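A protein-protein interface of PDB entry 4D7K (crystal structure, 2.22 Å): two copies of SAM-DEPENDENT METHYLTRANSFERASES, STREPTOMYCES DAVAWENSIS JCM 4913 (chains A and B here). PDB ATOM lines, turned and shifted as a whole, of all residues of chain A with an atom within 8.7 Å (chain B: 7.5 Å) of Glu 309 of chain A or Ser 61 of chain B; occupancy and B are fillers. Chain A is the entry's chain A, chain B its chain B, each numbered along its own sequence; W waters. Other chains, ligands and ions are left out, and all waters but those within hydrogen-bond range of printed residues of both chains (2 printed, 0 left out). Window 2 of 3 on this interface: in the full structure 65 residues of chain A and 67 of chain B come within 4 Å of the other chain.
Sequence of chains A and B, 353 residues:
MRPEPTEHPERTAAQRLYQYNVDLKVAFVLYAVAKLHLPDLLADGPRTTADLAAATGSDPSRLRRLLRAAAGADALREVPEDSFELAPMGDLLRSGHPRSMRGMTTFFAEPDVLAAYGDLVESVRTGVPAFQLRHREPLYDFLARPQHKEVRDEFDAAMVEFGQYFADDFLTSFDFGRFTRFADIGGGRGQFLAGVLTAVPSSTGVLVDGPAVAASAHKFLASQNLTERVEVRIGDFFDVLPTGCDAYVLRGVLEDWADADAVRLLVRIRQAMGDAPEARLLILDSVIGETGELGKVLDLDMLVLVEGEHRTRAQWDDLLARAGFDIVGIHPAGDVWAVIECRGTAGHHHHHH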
ATOM      1  N   SER A 123     -10.666   3.131   0.631  1.00  0.00           N
ATOM      2  CA  SER A 123     -11.783   2.206   0.810  1.00  0.00           C
ATOM      3  C   SER A 123     -11.300   0.789   1.141  1.00  0.00           C
ATOM      4  O   SER A 123     -11.817   0.145   2.056  1.00  0.00           O
ATOM      5  CB  SER A 123     -12.660   2.182  -0.444  1.00  0.00           C
ATOM      6  OG  SER A 123     -13.698   1.222  -0.325  1.00  0.00           O
ATOM      7  N   VAL A 124     -10.312   0.307   0.393  1.00  0.00           N
ATOM      8  CA  VAL A 124      -9.723  -1.002   0.661  1.00  0.00           C
ATOM      9  C   VAL A 124      -9.054  -1.002   2.035  1.00  0.00           C
ATOM     10  O   VAL A 124      -9.141  -1.981   2.782  1.00  0.00           O
ATOM     11  CB  VAL A 124      -8.699  -1.401  -0.428  1.00  0.00           C
ATOM     12  CG1 VAL A 124      -7.951  -2.656  -0.029  1.00  0.00           C
ATOM     13  CG2 VAL A 124      -9.402  -1.607  -1.764  1.00  0.00           C
ATOM     14  N   GLY A 127     -12.465  -0.135   4.719  1.00  0.00           N
ATOM     15  CA  GLY A 127     -13.568  -1.077   4.753  1.00  0.00           C
ATOM     16  C   GLY A 127     -14.871  -0.389   4.404  1.00  0.00           C
ATOM     17  O   GLY A 127     -15.906  -1.033   4.241  1.00  0.00           O
ATOM     18  N   VAL A 253     -31.455  -7.745  -6.097  1.00  0.00           N
ATOM     19  CA  VAL A 253     -32.276  -7.345  -4.963  1.00  0.00           C
ATOM     20  C   VAL A 253     -31.592  -7.662  -3.636  1.00  0.00           C
ATOM     21  O   VAL A 253     -31.431  -6.789  -2.782  1.00  0.00           O
ATOM     22  CB  VAL A 253     -33.650  -8.042  -5.001  1.00  0.00           C
ATOM     23  CG1 VAL A 253     -34.464  -7.680  -3.768  1.00  0.00           C
ATOM     24  CG2 VAL A 253     -34.397  -7.674  -6.278  1.00  0.00           C
ATOM     25  N   LEU A 254     -31.181  -8.915  -3.480  1.00  0.00           N
ATOM     26  CA  LEU A 254     -30.622  -9.398  -2.223  1.00  0.00           C
ATOM     27  C   LEU A 254     -29.174  -8.960  -2.028  1.00  0.00           C
ATOM     28  O   LEU A 254     -28.535  -9.328  -1.043  1.00  0.00           O
ATOM     29  CB  LEU A 254     -30.718 -10.921  -2.164  1.00  0.00           C
ATOM     30  CG  LEU A 254     -32.082 -11.480  -2.570  1.00  0.00           C
ATOM     31  CD1 LEU A 254     -32.063 -13.000  -2.587  1.00  0.00           C
ATOM     32  CD2 LEU A 254     -33.160 -10.960  -1.636  1.00  0.00           C
ATOM     33  N   GLU A 255     -28.665  -8.177  -2.973  1.00  0.00           N
ATOM     34  CA  GLU A 255     -27.288  -7.701  -2.925  1.00  0.00           C
ATOM     35  C   GLU A 255     -27.035  -6.782  -1.731  1.00  0.00           C
ATOM     36  O   GLU A 255     -25.942  -6.780  -1.162  1.00  0.00           O
ATOM     37  CB  GLU A 255     -26.937  -6.976  -4.226  1.00  0.00           C
ATOM     38  CG  GLU A 255     -26.886  -7.886  -5.440  1.00  0.00           C
ATOM     39  CD  GLU A 255     -26.897  -7.119  -6.745  1.00  0.00           C
ATOM     40  OE1 GLU A 255     -27.339  -5.950  -6.743  1.00  0.00           O
ATOM     41  OE2 GLU A 255     -26.465  -7.681  -7.773  1.00  0.00           O
ATOM     42  N   ASP A 256     -28.045  -6.005  -1.351  1.00  0.00           N
ATOM     43  CA  ASP A 256     -27.900  -5.067  -0.243  1.00  0.00           C
ATOM     44  C   ASP A 256     -28.813  -5.410   0.933  1.00  0.00           C
ATOM     45  O   ASP A 256     -28.874  -4.670   1.916  1.00  0.00           O
ATOM     46  CB  ASP A 256     -28.170  -3.636  -0.718  1.00  0.00           C
ATOM     47  CG  ASP A 256     -29.510  -3.495  -1.411  1.00  0.00           C
ATOM     48  OD1 ASP A 256     -30.023  -4.508  -1.928  1.00  0.00           O
ATOM     49  OD2 ASP A 256     -30.046  -2.368  -1.441  1.00  0.00           O
ATOM     50  N   TRP A 257     -29.523  -6.530   0.832  1.00  0.00           N
ATOM     51  CA  TRP A 257     -30.328  -7.019   1.947  1.00  0.00           C
ATOM     52  C   TRP A 257     -29.465  -7.812   2.921  1.00  0.00           C
ATOM     53  O   TRP A 257     -28.551  -8.529   2.511  1.00  0.00           O
ATOM     54  CB  TRP A 257     -31.487  -7.891   1.453  1.00  0.00           C
ATOM     55  CG  TRP A 257     -32.672  -7.127   0.951  1.00  0.00           C
ATOM     56  CD1 TRP A 257     -32.657  -6.000   0.186  1.00  0.00           C
ATOM     57  CD2 TRP A 257     -34.053  -7.430   1.189  1.00  0.00           C
ATOM     58  NE1 TRP A 257     -33.941  -5.585  -0.075  1.00  0.00           N
ATOM     59  CE2 TRP A 257     -34.818  -6.447   0.533  1.00  0.00           C
ATOM     60  CE3 TRP A 257     -34.717  -8.440   1.893  1.00  0.00           C
ATOM     61  CZ2 TRP A 257     -36.210  -6.441   0.558  1.00  0.00           C
ATOM     62  CZ3 TRP A 257     -36.101  -8.432   1.918  1.00  0.00           C
ATOM     63  CH2 TRP A 257     -36.832  -7.442   1.254  1.00  0.00           C
ATOM     64  N   ASP A 259     -28.708 -10.787   5.814  1.00  0.00           N
ATOM     65  CA  ASP A 259     -29.024 -12.212   5.827  1.00  0.00           C
ATOM     66  C   ASP A 259     -30.391 -12.463   6.445  1.00  0.00           C
ATOM     67  O   ASP A 259     -31.233 -13.135   5.849  1.00  0.00           O
ATOM     68  CB  ASP A 259     -27.955 -13.000   6.587  1.00  0.00           C
ATOM     69  CG  ASP A 259     -26.667 -13.144   5.801  1.00  0.00           C
ATOM     70  OD1 ASP A 259     -26.705 -12.977   4.564  1.00  0.00           O
ATOM     71  OD2 ASP A 259     -25.620 -13.431   6.419  1.00  0.00           O
ATOM     72  N   ASP A 285     -27.667 -12.865 -10.848  1.00  0.00           N
ATOM     73  CA  ASP A 285     -26.616 -12.148 -10.142  1.00  0.00           C
ATOM     74  C   ASP A 285     -25.242 -12.546 -10.664  1.00  0.00           C
ATOM     75  O   ASP A 285     -25.117 -13.454 -11.485  1.00  0.00           O
ATOM     76  CB  ASP A 285     -26.705 -12.422  -8.635  1.00  0.00           C
ATOM     77  CG  ASP A 285     -26.073 -11.323  -7.793  1.00  0.00           C
ATOM     78  OD1 ASP A 285     -25.398 -10.436  -8.358  1.00  0.00           O
ATOM     79  OD2 ASP A 285     -26.246 -11.350  -6.556  1.00  0.00           O
ATOM     80  N   SER A 286     -24.216 -11.846 -10.193  1.00  0.00           N
ATOM     81  CA  SER A 286     -22.841 -12.266 -10.407  1.00  0.00           C
ATOM     82  C   SER A 286     -22.411 -13.105  -9.209  1.00  0.00           C
ATOM     83  O   SER A 286     -22.583 -12.693  -8.062  1.00  0.00           O
ATOM     84  CB  SER A 286     -21.920 -11.061 -10.590  1.00  0.00           C
ATOM     85  OG  SER A 286     -20.585 -11.472 -10.822  1.00  0.00           O
ATOM     86  N   ILE A 288     -19.533 -14.870  -7.046  1.00  0.00           N
ATOM     87  CA  ILE A 288     -18.113 -14.904  -6.714  1.00  0.00           C
ATOM     88  C   ILE A 288     -17.563 -16.316  -6.848  1.00  0.00           C
ATOM     89  O   ILE A 288     -18.093 -17.255  -6.256  1.00  0.00           O
ATOM     90  CB  ILE A 288     -17.848 -14.394  -5.281  1.00  0.00           C
ATOM     91  CG1 ILE A 288     -18.370 -12.962  -5.107  1.00  0.00           C
ATOM     92  CG2 ILE A 288     -16.361 -14.476  -4.951  1.00  0.00           C
ATOM     93  CD1 ILE A 288     -17.604 -11.939  -5.911  1.00  0.00           C
ATOM     94  N   ASP A 299     -16.898  -5.935 -10.216  1.00  0.00           N
ATOM     95  CA  ASP A 299     -17.152  -5.897  -8.778  1.00  0.00           C
ATOM     96  C   ASP A 299     -16.544  -4.637  -8.165  1.00  0.00           C
ATOM     97  O   ASP A 299     -16.859  -4.272  -7.031  1.00  0.00           O
ATOM     98  CB  ASP A 299     -16.598  -7.142  -8.082  1.00  0.00           C
ATOM     99  CG  ASP A 299     -17.081  -7.267  -6.634  1.00  0.00           C
ATOM    100  OD1 ASP A 299     -18.196  -6.794  -6.332  1.00  0.00           O
ATOM    101  OD2 ASP A 299     -16.350  -7.836  -5.798  1.00  0.00           O
ATOM    102  N   MET A 302     -19.230  -2.168  -7.258  1.00  0.00           N
ATOM    103  CA  MET A 302     -19.835  -2.487  -5.971  1.00  0.00           C
ATOM    104  C   MET A 302     -18.957  -1.995  -4.833  1.00  0.00           C
ATOM    105  O   MET A 302     -19.451  -1.503  -3.826  1.00  0.00           O
ATOM    106  CB  MET A 302     -20.059  -3.993  -5.849  1.00  0.00           C
ATOM    107  CG  MET A 302     -20.838  -4.589  -7.003  1.00  0.00           C
ATOM    108  SD  MET A 302     -22.609  -4.482  -6.727  1.00  0.00           S
ATOM    109  CE  MET A 302     -22.771  -5.649  -5.372  1.00  0.00           C
ATOM    110  N   LEU A 303     -17.648  -2.128  -5.011  1.00  0.00           N
ATOM    111  CA  LEU A 303     -16.682  -1.747  -3.988  1.00  0.00           C
ATOM    112  C   LEU A 303     -16.624  -0.232  -3.811  1.00  0.00           C
ATOM    113  O   LEU A 303     -16.456   0.268  -2.702  1.00  0.00           O
ATOM    114  CB  LEU A 303     -15.301  -2.291  -4.356  1.00  0.00           C
ATOM    115  CG  LEU A 303     -14.302  -2.583  -3.241  1.00  0.00           C
ATOM    116  CD1 LEU A 303     -13.327  -3.640  -3.712  1.00  0.00           C
ATOM    117  CD2 LEU A 303     -13.557  -1.324  -2.851  1.00  0.00           C
ATOM    118  N   VAL A 306     -21.422   1.152  -3.568  1.00  0.00           N
ATOM    119  CA  VAL A 306     -22.363   0.685  -2.557  1.00  0.00           C
ATOM    120  C   VAL A 306     -21.724  -0.187  -1.480  1.00  0.00           C
ATOM    121  O   VAL A 306     -20.547  -0.539  -1.558  1.00  0.00           O
ATOM    122  CB  VAL A 306     -23.510  -0.096  -3.205  1.00  0.00           C
ATOM    123  CG1 VAL A 306     -24.274   0.803  -4.160  1.00  0.00           C
ATOM    124  CG2 VAL A 306     -22.968  -1.308  -3.928  1.00  0.00           C
ATOM    125  N   GLU A 307     -22.517  -0.527  -0.470  1.00  0.00           N
ATOM    126  CA  GLU A 307     -22.029  -1.296   0.669  1.00  0.00           C
ATOM    127  C   GLU A 307     -22.304  -2.788   0.485  1.00  0.00           C
ATOM    128  O   GLU A 307     -21.661  -3.633   1.111  1.00  0.00           O
ATOM    129  CB  GLU A 307     -22.672  -0.779   1.959  1.00  0.00           C
ATOM    130  CG  GLU A 307     -21.987  -1.235   3.237  1.00  0.00           C
ATOM    131  CD  GLU A 307     -22.627  -2.472   3.828  1.00  0.00           C
ATOM    132  OE1 GLU A 307     -23.683  -2.898   3.315  1.00  0.00           O
ATOM    133  OE2 GLU A 307     -22.077  -3.017   4.810  1.00  0.00           O
ATOM    134  N   GLY A 308     -23.256  -3.106  -0.387  1.00  0.00           N
ATOM    135  CA  GLY A 308     -23.624  -4.484  -0.653  1.00  0.00           C
ATOM    136  C   GLY A 308     -22.538  -5.271  -1.365  1.00  0.00           C
ATOM    137  O   GLY A 308     -21.606  -4.696  -1.932  1.00  0.00           O
ATOM    138  N   GLU A 309     -22.671  -6.594  -1.347  1.00  0.00           N
ATOM    139  CA  GLU A 309     -21.658  -7.475  -1.911  1.00  0.00           C
ATOM    140  C   GLU A 309     -22.279  -8.687  -2.616  1.00  0.00           C
ATOM    141  O   GLU A 309     -23.363  -9.142  -2.250  1.00  0.00           O
ATOM    142  CB  GLU A 309     -20.706  -7.934  -0.805  1.00  0.00           C
ATOM    143  CG  GLU A 309     -19.399  -8.535  -1.293  1.00  0.00           C
ATOM    144  CD  GLU A 309     -18.477  -8.920  -0.150  1.00  0.00           C
ATOM    145  OE1 GLU A 309     -18.936  -8.922   1.012  1.00  0.00           O
ATOM    146  OE2 GLU A 309     -17.293  -9.221  -0.411  1.00  0.00           O
ATOM    147  N   HIS A 310     -21.592  -9.198  -3.635  1.00  0.00           N
ATOM    148  CA  HIS A 310     -22.012 -10.427  -4.294  1.00  0.00           C
ATOM    149  C   HIS A 310     -21.705 -11.609  -3.393  1.00  0.00           C
ATOM    150  O   HIS A 310     -20.811 -11.533  -2.549  1.00  0.00           O
ATOM    151  CB  HIS A 310     -21.316 -10.596  -5.644  1.00  0.00           C
ATOM    152  CG  HIS A 310     -21.652  -9.529  -6.636  1.00  0.00           C
ATOM    153  ND1 HIS A 310     -22.942  -9.291  -7.065  1.00  0.00           N
ATOM    154  CD2 HIS A 310     -20.868  -8.642  -7.295  1.00  0.00           C
ATOM    155  CE1 HIS A 310     -22.937  -8.299  -7.938  1.00  0.00           C
ATOM    156  NE2 HIS A 310     -21.691  -7.889  -8.095  1.00  0.00           N
ATOM    157  N   ARG A 311     -22.442 -12.701  -3.564  1.00  0.00           N
ATOM    158  CA  ARG A 311     -22.259 -13.868  -2.710  1.00  0.00           C
ATOM    159  C   ARG A 311     -21.616 -15.043  -3.447  1.00  0.00           C
ATOM    160  O   ARG A 311     -21.793 -15.208  -4.658  1.00  0.00           O
ATOM    161  CB  ARG A 311     -23.602 -14.301  -2.111  1.00  0.00           C
ATOM    162  CG  ARG A 311     -24.152 -13.371  -1.030  1.00  0.00           C
ATOM    163  CD  ARG A 311     -25.490 -13.885  -0.505  1.00  0.00           C
ATOM    164  NE  ARG A 311     -25.979 -13.152   0.662  1.00  0.00           N
ATOM    165  CZ  ARG A 311     -26.813 -12.116   0.603  1.00  0.00           C
ATOM    166  NH1 ARG A 311     -27.252 -11.678  -0.569  1.00  0.00           N
ATOM    167  NH2 ARG A 311     -27.207 -11.514   1.719  1.00  0.00           N
ATOM    168  N   THR A 312     -20.854 -15.849  -2.709  1.00  0.00           N
ATOM    169  CA  THR A 312     -20.310 -17.087  -3.251  1.00  0.00           C
ATOM    170  C   THR A 312     -21.415 -18.126  -3.290  1.00  0.00           C
ATOM    171  O   THR A 312     -22.504 -17.893  -2.770  1.00  0.00           O
ATOM    172  CB  THR A 312     -19.142 -17.634  -2.414  1.00  0.00           C
ATOM    173  OG1 THR A 312     -19.625 -18.023  -1.122  1.00  0.00           O
ATOM    174  CG2 THR A 312     -18.052 -16.592  -2.258  1.00  0.00           C
ATOM    175  N   GLN A 315     -22.278 -19.451   0.210  1.00  0.00           N
ATOM    176  CA  GLN A 315     -23.104 -18.470   0.901  1.00  0.00           C
ATOM    177  C   GLN A 315     -24.560 -18.568   0.459  1.00  0.00           C
ATOM    178  O   GLN A 315     -25.474 -18.510   1.287  1.00  0.00           O
ATOM    179  CB  GLN A 315     -22.566 -17.060   0.662  1.00  0.00           C
ATOM    180  CG  GLN A 315     -21.252 -16.778   1.368  1.00  0.00           C
ATOM    181  CD  GLN A 315     -20.685 -15.415   1.025  1.00  0.00           C
ATOM    182  OE1 GLN A 315     -20.563 -15.057  -0.148  1.00  0.00           O
ATOM    183  NE2 GLN A 315     -20.342 -14.643   2.049  1.00  0.00           N
ATOM    184  N   TRP A 316     -24.769 -18.727  -0.846  1.00  0.00           N
ATOM    185  CA  TRP A 316     -26.115 -18.878  -1.390  1.00  0.00           C
ATOM    186  C   TRP A 316     -26.750 -20.173  -0.915  1.00  0.00           C
ATOM    187  O   TRP A 316     -27.938 -20.206  -0.599  1.00  0.00           O
ATOM    188  CB  TRP A 316     -26.100 -18.836  -2.919  1.00  0.00           C
ATOM    189  CG  TRP A 316     -26.068 -17.449  -3.490  1.00  0.00           C
ATOM    190  CD1 TRP A 316     -25.060 -16.886  -4.221  1.00  0.00           C
ATOM    191  CD2 TRP A 316     -27.089 -16.448  -3.377  1.00  0.00           C
ATOM    192  NE1 TRP A 316     -25.392 -15.599  -4.574  1.00  0.00           N
ATOM    193  CE2 TRP A 316     -26.632 -15.305  -4.068  1.00  0.00           C
ATOM    194  CE3 TRP A 316     -28.346 -16.406  -2.761  1.00  0.00           C
ATOM    195  CZ2 TRP A 316     -27.385 -14.135  -4.160  1.00  0.00           C
ATOM    196  CZ3 TRP A 316     -29.093 -15.244  -2.854  1.00  0.00           C
ATOM    197  CH2 TRP A 316     -28.608 -14.123  -3.548  1.00  0.00           C
ATOM    198  N   THR B  49      -3.681 -13.462   0.716  1.00  0.00           N
ATOM    199  CA  THR B  49      -4.489 -12.271   0.962  1.00  0.00           C
ATOM    200  C   THR B  49      -4.234 -11.700   2.355  1.00  0.00           C
ATOM    201  O   THR B  49      -3.996 -10.500   2.503  1.00  0.00           O
ATOM    202  CB  THR B  49      -5.990 -12.572   0.817  1.00  0.00           C
ATOM    203  OG1 THR B  49      -6.268 -12.971  -0.530  1.00  0.00           O
ATOM    204  CG2 THR B  49      -6.818 -11.342   1.159  1.00  0.00           C
ATOM    205  N   ALA B  53      -2.735  -8.176   3.221  1.00  0.00           N
ATOM    206  CA  ALA B  53      -3.536  -7.309   4.082  1.00  0.00           C
ATOM    207  C   ALA B  53      -2.674  -6.662   5.165  1.00  0.00           C
ATOM    208  O   ALA B  53      -2.728  -5.450   5.372  1.00  0.00           O
ATOM    209  CB  ALA B  53      -4.677  -8.095   4.716  1.00  0.00           C
ATOM    210  N   SER B  58      -4.793  -3.248   5.098  1.00  0.00           N
ATOM    211  CA  SER B  58      -6.092  -3.243   4.432  1.00  0.00           C
ATOM    212  C   SER B  58      -7.082  -4.225   5.045  1.00  0.00           C
ATOM    213  O   SER B  58      -6.696  -5.188   5.711  1.00  0.00           O
ATOM    214  CB  SER B  58      -5.926  -3.571   2.945  1.00  0.00           C
ATOM    215  OG  SER B  58      -5.050  -2.663   2.302  1.00  0.00           O
ATOM    216  N   ASP B  59      -8.367  -3.975   4.810  1.00  0.00           N
ATOM    217  CA  ASP B  59      -9.405  -4.947   5.130  1.00  0.00           C
ATOM    218  C   ASP B  59      -9.244  -6.148   4.206  1.00  0.00           C
ATOM    219  O   ASP B  59      -9.331  -6.005   2.987  1.00  0.00           O
ATOM    220  CB  ASP B  59     -10.799  -4.325   4.983  1.00  0.00           C
ATOM    221  CG  ASP B  59     -11.913  -5.361   5.004  1.00  0.00           C
ATOM    222  OD1 ASP B  59     -11.826  -6.331   5.786  1.00  0.00           O
ATOM    223  OD2 ASP B  59     -12.882  -5.204   4.232  1.00  0.00           O
ATOM    224  N   PRO B  60      -8.992  -7.333   4.781  1.00  0.00           N
ATOM    225  CA  PRO B  60      -8.751  -8.555   4.002  1.00  0.00           C
ATOM    226  C   PRO B  60      -9.838  -8.854   2.964  1.00  0.00           C
ATOM    227  O   PRO B  60      -9.516  -9.247   1.842  1.00  0.00           O
ATOM    228  CB  PRO B  60      -8.714  -9.646   5.075  1.00  0.00           C
ATOM    229  CG  PRO B  60      -8.256  -8.940   6.301  1.00  0.00           C
ATOM    230  CD  PRO B  60      -8.861  -7.569   6.230  1.00  0.00           C
ATOM    231  N   SER B  61     -11.102  -8.658   3.328  1.00  0.00           N
ATOM    232  CA  SER B  61     -12.206  -9.003   2.439  1.00  0.00           C
ATOM    233  C   SER B  61     -12.282  -8.076   1.232  1.00  0.00           C
ATOM    234  O   SER B  61     -12.637  -8.505   0.134  1.00  0.00           O
ATOM    235  CB  SER B  61     -13.534  -8.976   3.190  1.00  0.00           C
ATOM    236  OG  SER B  61     -14.594  -9.361   2.332  1.00  0.00           O
ATOM    237  N   ARG B  62     -11.951  -6.805   1.433  1.00  0.00           N
ATOM    238  CA  ARG B  62     -11.996  -5.845   0.339  1.00  0.00           C
ATOM    239  C   ARG B  62     -10.693  -5.817  -0.456  1.00  0.00           C
ATOM    240  O   ARG B  62     -10.687  -5.423  -1.627  1.00  0.00           O
ATOM    241  CB  ARG B  62     -12.331  -4.453   0.869  1.00  0.00           C
ATOM    242  CG  ARG B  62     -13.788  -4.327   1.276  1.00  0.00           C
ATOM    243  CD  ARG B  62     -14.185  -2.907   1.630  1.00  0.00           C
ATOM    244  NE  ARG B  62     -15.625  -2.719   1.482  1.00  0.00           N
ATOM    245  CZ  ARG B  62     -16.182  -1.913   0.585  1.00  0.00           C
ATOM    246  NH1 ARG B  62     -15.418  -1.200  -0.230  1.00  0.00           N
ATOM    247  NH2 ARG B  62     -17.501  -1.807   0.512  1.00  0.00           N
ATOM    248  N   LEU B  63      -9.597  -6.233   0.173  1.00  0.00           N
ATOM    249  CA  LEU B  63      -8.329  -6.354  -0.535  1.00  0.00           C
ATOM    250  C   LEU B  63      -8.439  -7.468  -1.562  1.00  0.00           C
ATOM    251  O   LEU B  63      -8.031  -7.308  -2.711  1.00  0.00           O
ATOM    252  CB  LEU B  63      -7.167  -6.636   0.421  1.00  0.00           C
ATOM    253  CG  LEU B  63      -5.830  -6.788  -0.314  1.00  0.00           C
ATOM    254  CD1 LEU B  63      -5.391  -5.464  -0.930  1.00  0.00           C
ATOM    255  CD2 LEU B  63      -4.748  -7.351   0.586  1.00  0.00           C
ATOM    256  N   ARG B  64      -9.002  -8.593  -1.131  1.00  0.00           N
ATOM    257  CA  ARG B  64      -9.208  -9.750  -1.996  1.00  0.00           C
ATOM    258  C   ARG B  64     -10.018  -9.404  -3.245  1.00  0.00           C
ATOM    259  O   ARG B  64      -9.754  -9.922  -4.329  1.00  0.00           O
ATOM    260  CB  ARG B  64      -9.907 -10.870  -1.220  1.00  0.00           C
ATOM    261  CG  ARG B  64     -10.136 -12.132  -2.035  1.00  0.00           C
ATOM    262  CD  ARG B  64     -10.805 -13.226  -1.224  1.00  0.00           C
ATOM    263  NE  ARG B  64     -10.028 -13.612  -0.049  1.00  0.00           N
ATOM    264  CZ  ARG B  64     -10.355 -13.272   1.192  1.00  0.00           C
ATOM    265  NH1 ARG B  64     -11.441 -12.541   1.406  1.00  0.00           N
ATOM    266  NH2 ARG B  64      -9.604 -13.662   2.214  1.00  0.00           N
ATOM    267  N   ARG B  65     -11.003  -8.527  -3.089  1.00  0.00           N
ATOM    268  CA  ARG B  65     -11.849  -8.126  -4.208  1.00  0.00           C
ATOM    269  C   ARG B  65     -11.086  -7.246  -5.198  1.00  0.00           C
ATOM    270  O   ARG B  65     -11.293  -7.329  -6.411  1.00  0.00           O
ATOM    271  CB  ARG B  65     -13.095  -7.409  -3.689  1.00  0.00           C
ATOM    272  CG  ARG B  65     -14.000  -8.312  -2.863  1.00  0.00           C
ATOM    273  CD  ARG B  65     -15.074  -7.520  -2.146  1.00  0.00           C
ATOM    274  NE  ARG B  65     -15.899  -6.766  -3.083  1.00  0.00           N
ATOM    275  CZ  ARG B  65     -16.920  -5.993  -2.728  1.00  0.00           C
ATOM    276  NH1 ARG B  65     -17.249  -5.869  -1.450  1.00  0.00           N
ATOM    277  NH2 ARG B  65     -17.612  -5.343  -3.653  1.00  0.00           N
ATOM    278  N   LEU B  66     -10.189  -6.418  -4.675  1.00  0.00           N
ATOM    279  CA  LEU B  66      -9.323  -5.600  -5.512  1.00  0.00           C
ATOM    280  C   LEU B  66      -8.295  -6.464  -6.248  1.00  0.00           C
ATOM    281  O   LEU B  66      -8.061  -6.290  -7.447  1.00  0.00           O
ATOM    282  CB  LEU B  66      -8.621  -4.543  -4.659  1.00  0.00           C
ATOM    283  CG  LEU B  66      -7.656  -3.582  -5.351  1.00  0.00           C
ATOM    284  CD1 LEU B  66      -8.393  -2.692  -6.326  1.00  0.00           C
ATOM    285  CD2 LEU B  66      -6.940  -2.745  -4.305  1.00  0.00           C
ATOM    286  N   ARG B  68      -8.531  -9.612  -6.939  1.00  0.00           N
ATOM    287  CA  ARG B  68      -9.277 -10.407  -7.904  1.00  0.00           C
ATOM    288  C   ARG B  68      -9.607  -9.611  -9.171  1.00  0.00           C
ATOM    289  O   ARG B  68      -9.560 -10.151 -10.273  1.00  0.00           O
ATOM    290  CB  ARG B  68     -10.554 -10.926  -7.258  1.00  0.00           C
ATOM    291  CG  ARG B  68     -11.192 -12.075  -7.981  1.00  0.00           C
ATOM    292  CD  ARG B  68     -12.501 -12.445  -7.314  1.00  0.00           C
ATOM    293  NE  ARG B  68     -12.316 -13.088  -6.016  1.00  0.00           N
ATOM    294  CZ  ARG B  68     -12.951 -12.723  -4.905  1.00  0.00           C
ATOM    295  NH1 ARG B  68     -13.809 -11.711  -4.927  1.00  0.00           N
ATOM    296  NH2 ARG B  68     -12.732 -13.370  -3.770  1.00  0.00           N
HETATM  297  O   HOH W   1     -15.558  -7.292   1.159  1.00  0.00           O
HETATM  298  O   HOH W   2     -14.889 -10.204  -6.500  1.00  0.00           O
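The backbone carbonyl oxygen (O) of Val 124 of chain A is in hydrogen-bond range of the backbone NH (N) of Asp 59 of chain B, at 2.9 Å.
NE of Arg 62 of chain B is in hydrogen-bond range of O of Gly 127 of chain A, 3.2 Å away.
N of Leu 303 of chain A lies close to NH2 of Arg 65 of chain B (3.5 Å).
The side-chain hydroxyl (OG) of Ser 123 of chain A sits at hydrogen-bond distance from the guanidinium group (NH1) of Arg 62 of chain B, 3.0 Å away.
The backbone carbonyl oxygen (O) of Leu 303 of chain A is in hydrogen-bond range of the guanidinium group (NH1) of Arg 62 of chain B (3.1 Å).
OD2 of Asp 299 of chain A lies within salt-bridge range of NE of Arg 65 of chain B, 3.0 Å away.
OE2 of Glu 309 of chain A lies within salt-bridge range of NH1 of Arg 65 of chain B (3.5 Å).
The backbone NH (N) of Ser 61 of chain B sits close to the side-chain carboxylate (OD1) of Asp 59 of chain B (3.5 Å).
The backbone carbonyl oxygen (O) of Ala 53 of chain B is in hydrogen-bond range of the backbone NH (N) of Ser 58 of chain B (3.0 Å).
SD of Met 302 of chain A sits close to NE2 of His 310 of chain A, 3.8 Å away.
The backbone NH (N) of Glu 309 of chain A is in hydrogen-bond range of the backbone carbonyl oxygen (O) of Glu 255 of chain A (3.3 Å).
The side-chain carboxylate (OD2) of Asp 59 of chain B lies close to the backbone NH (N) of Arg 62 of chain B (3.4 Å).
The backbone carbonyl oxygen of Arg 311 of chain A is in hydrogen-bond range of the backbone NH of Ile 288 of chain A, at 3.3 Å.
Val 124 of chain A touches Ser 58 of chain B (O to CB, 3.6 Å).
Leu 63 of chain B touches Val 124 of chain A (CA to CG1, 3.8 Å).
CD2 of Leu 66 of chain B touches CG2 of Val 124 of chain A (3.7 Å).
Arg 68 of chain B touches Ile 288 of chain A.
Met 302 of chain A touches Arg 65 of chain B (CB to NH2, 3.6 Å).
Arg 62 of chain B touches Val 306 of chain A (NH2 to O, 3.9 Å).
Ser 61 of chain B touches Glu 309 of chain A.
Printed residues of chain B within 4 Å of Ile 288 of chain A: Arg 68 (3.8 Å).
Of the printed residues of chain A, Asp 59 of chain B touches Val 124.
No residue of chain A comes within 4 Å of Pro 60 of chain B.
Ser 61 of chain B touches just one residue of chain A: Glu 309 (3.9 Å).
The nearest residue of chain A that does not touch Ser 61 of chain B is Leu 303 of chain A (6.2 Å).
The nearest printed residue of chain B that does not touch Gly 127 of chain A is Asp 59 of chain B (4.2 Å).
Of the 12 printed residues of chain B, 8 touch a printed residue of chain A.
Hydrophobic or aromatic side chains of chain B that line the printed part of chain A: Leu 63 and Leu 66.
Among the printed residues, 14 pairs touch across the chains.
No position is printed for both chains.
Water W2 lies within hydrogen-bond range of NH1 of Arg 68 of chain B (2.4 Å) and OD2 of Asp 299 of chain A (2.9 Å).
Water W1 lies within hydrogen-bond range of the side-chain hydroxyl of Ser 61 of chain B (2.6 Å), the side-chain carboxylate of Glu 309 of chain A (3.0 Å) and the guanidinium group of Arg 65 of chain B (3.4 Å).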
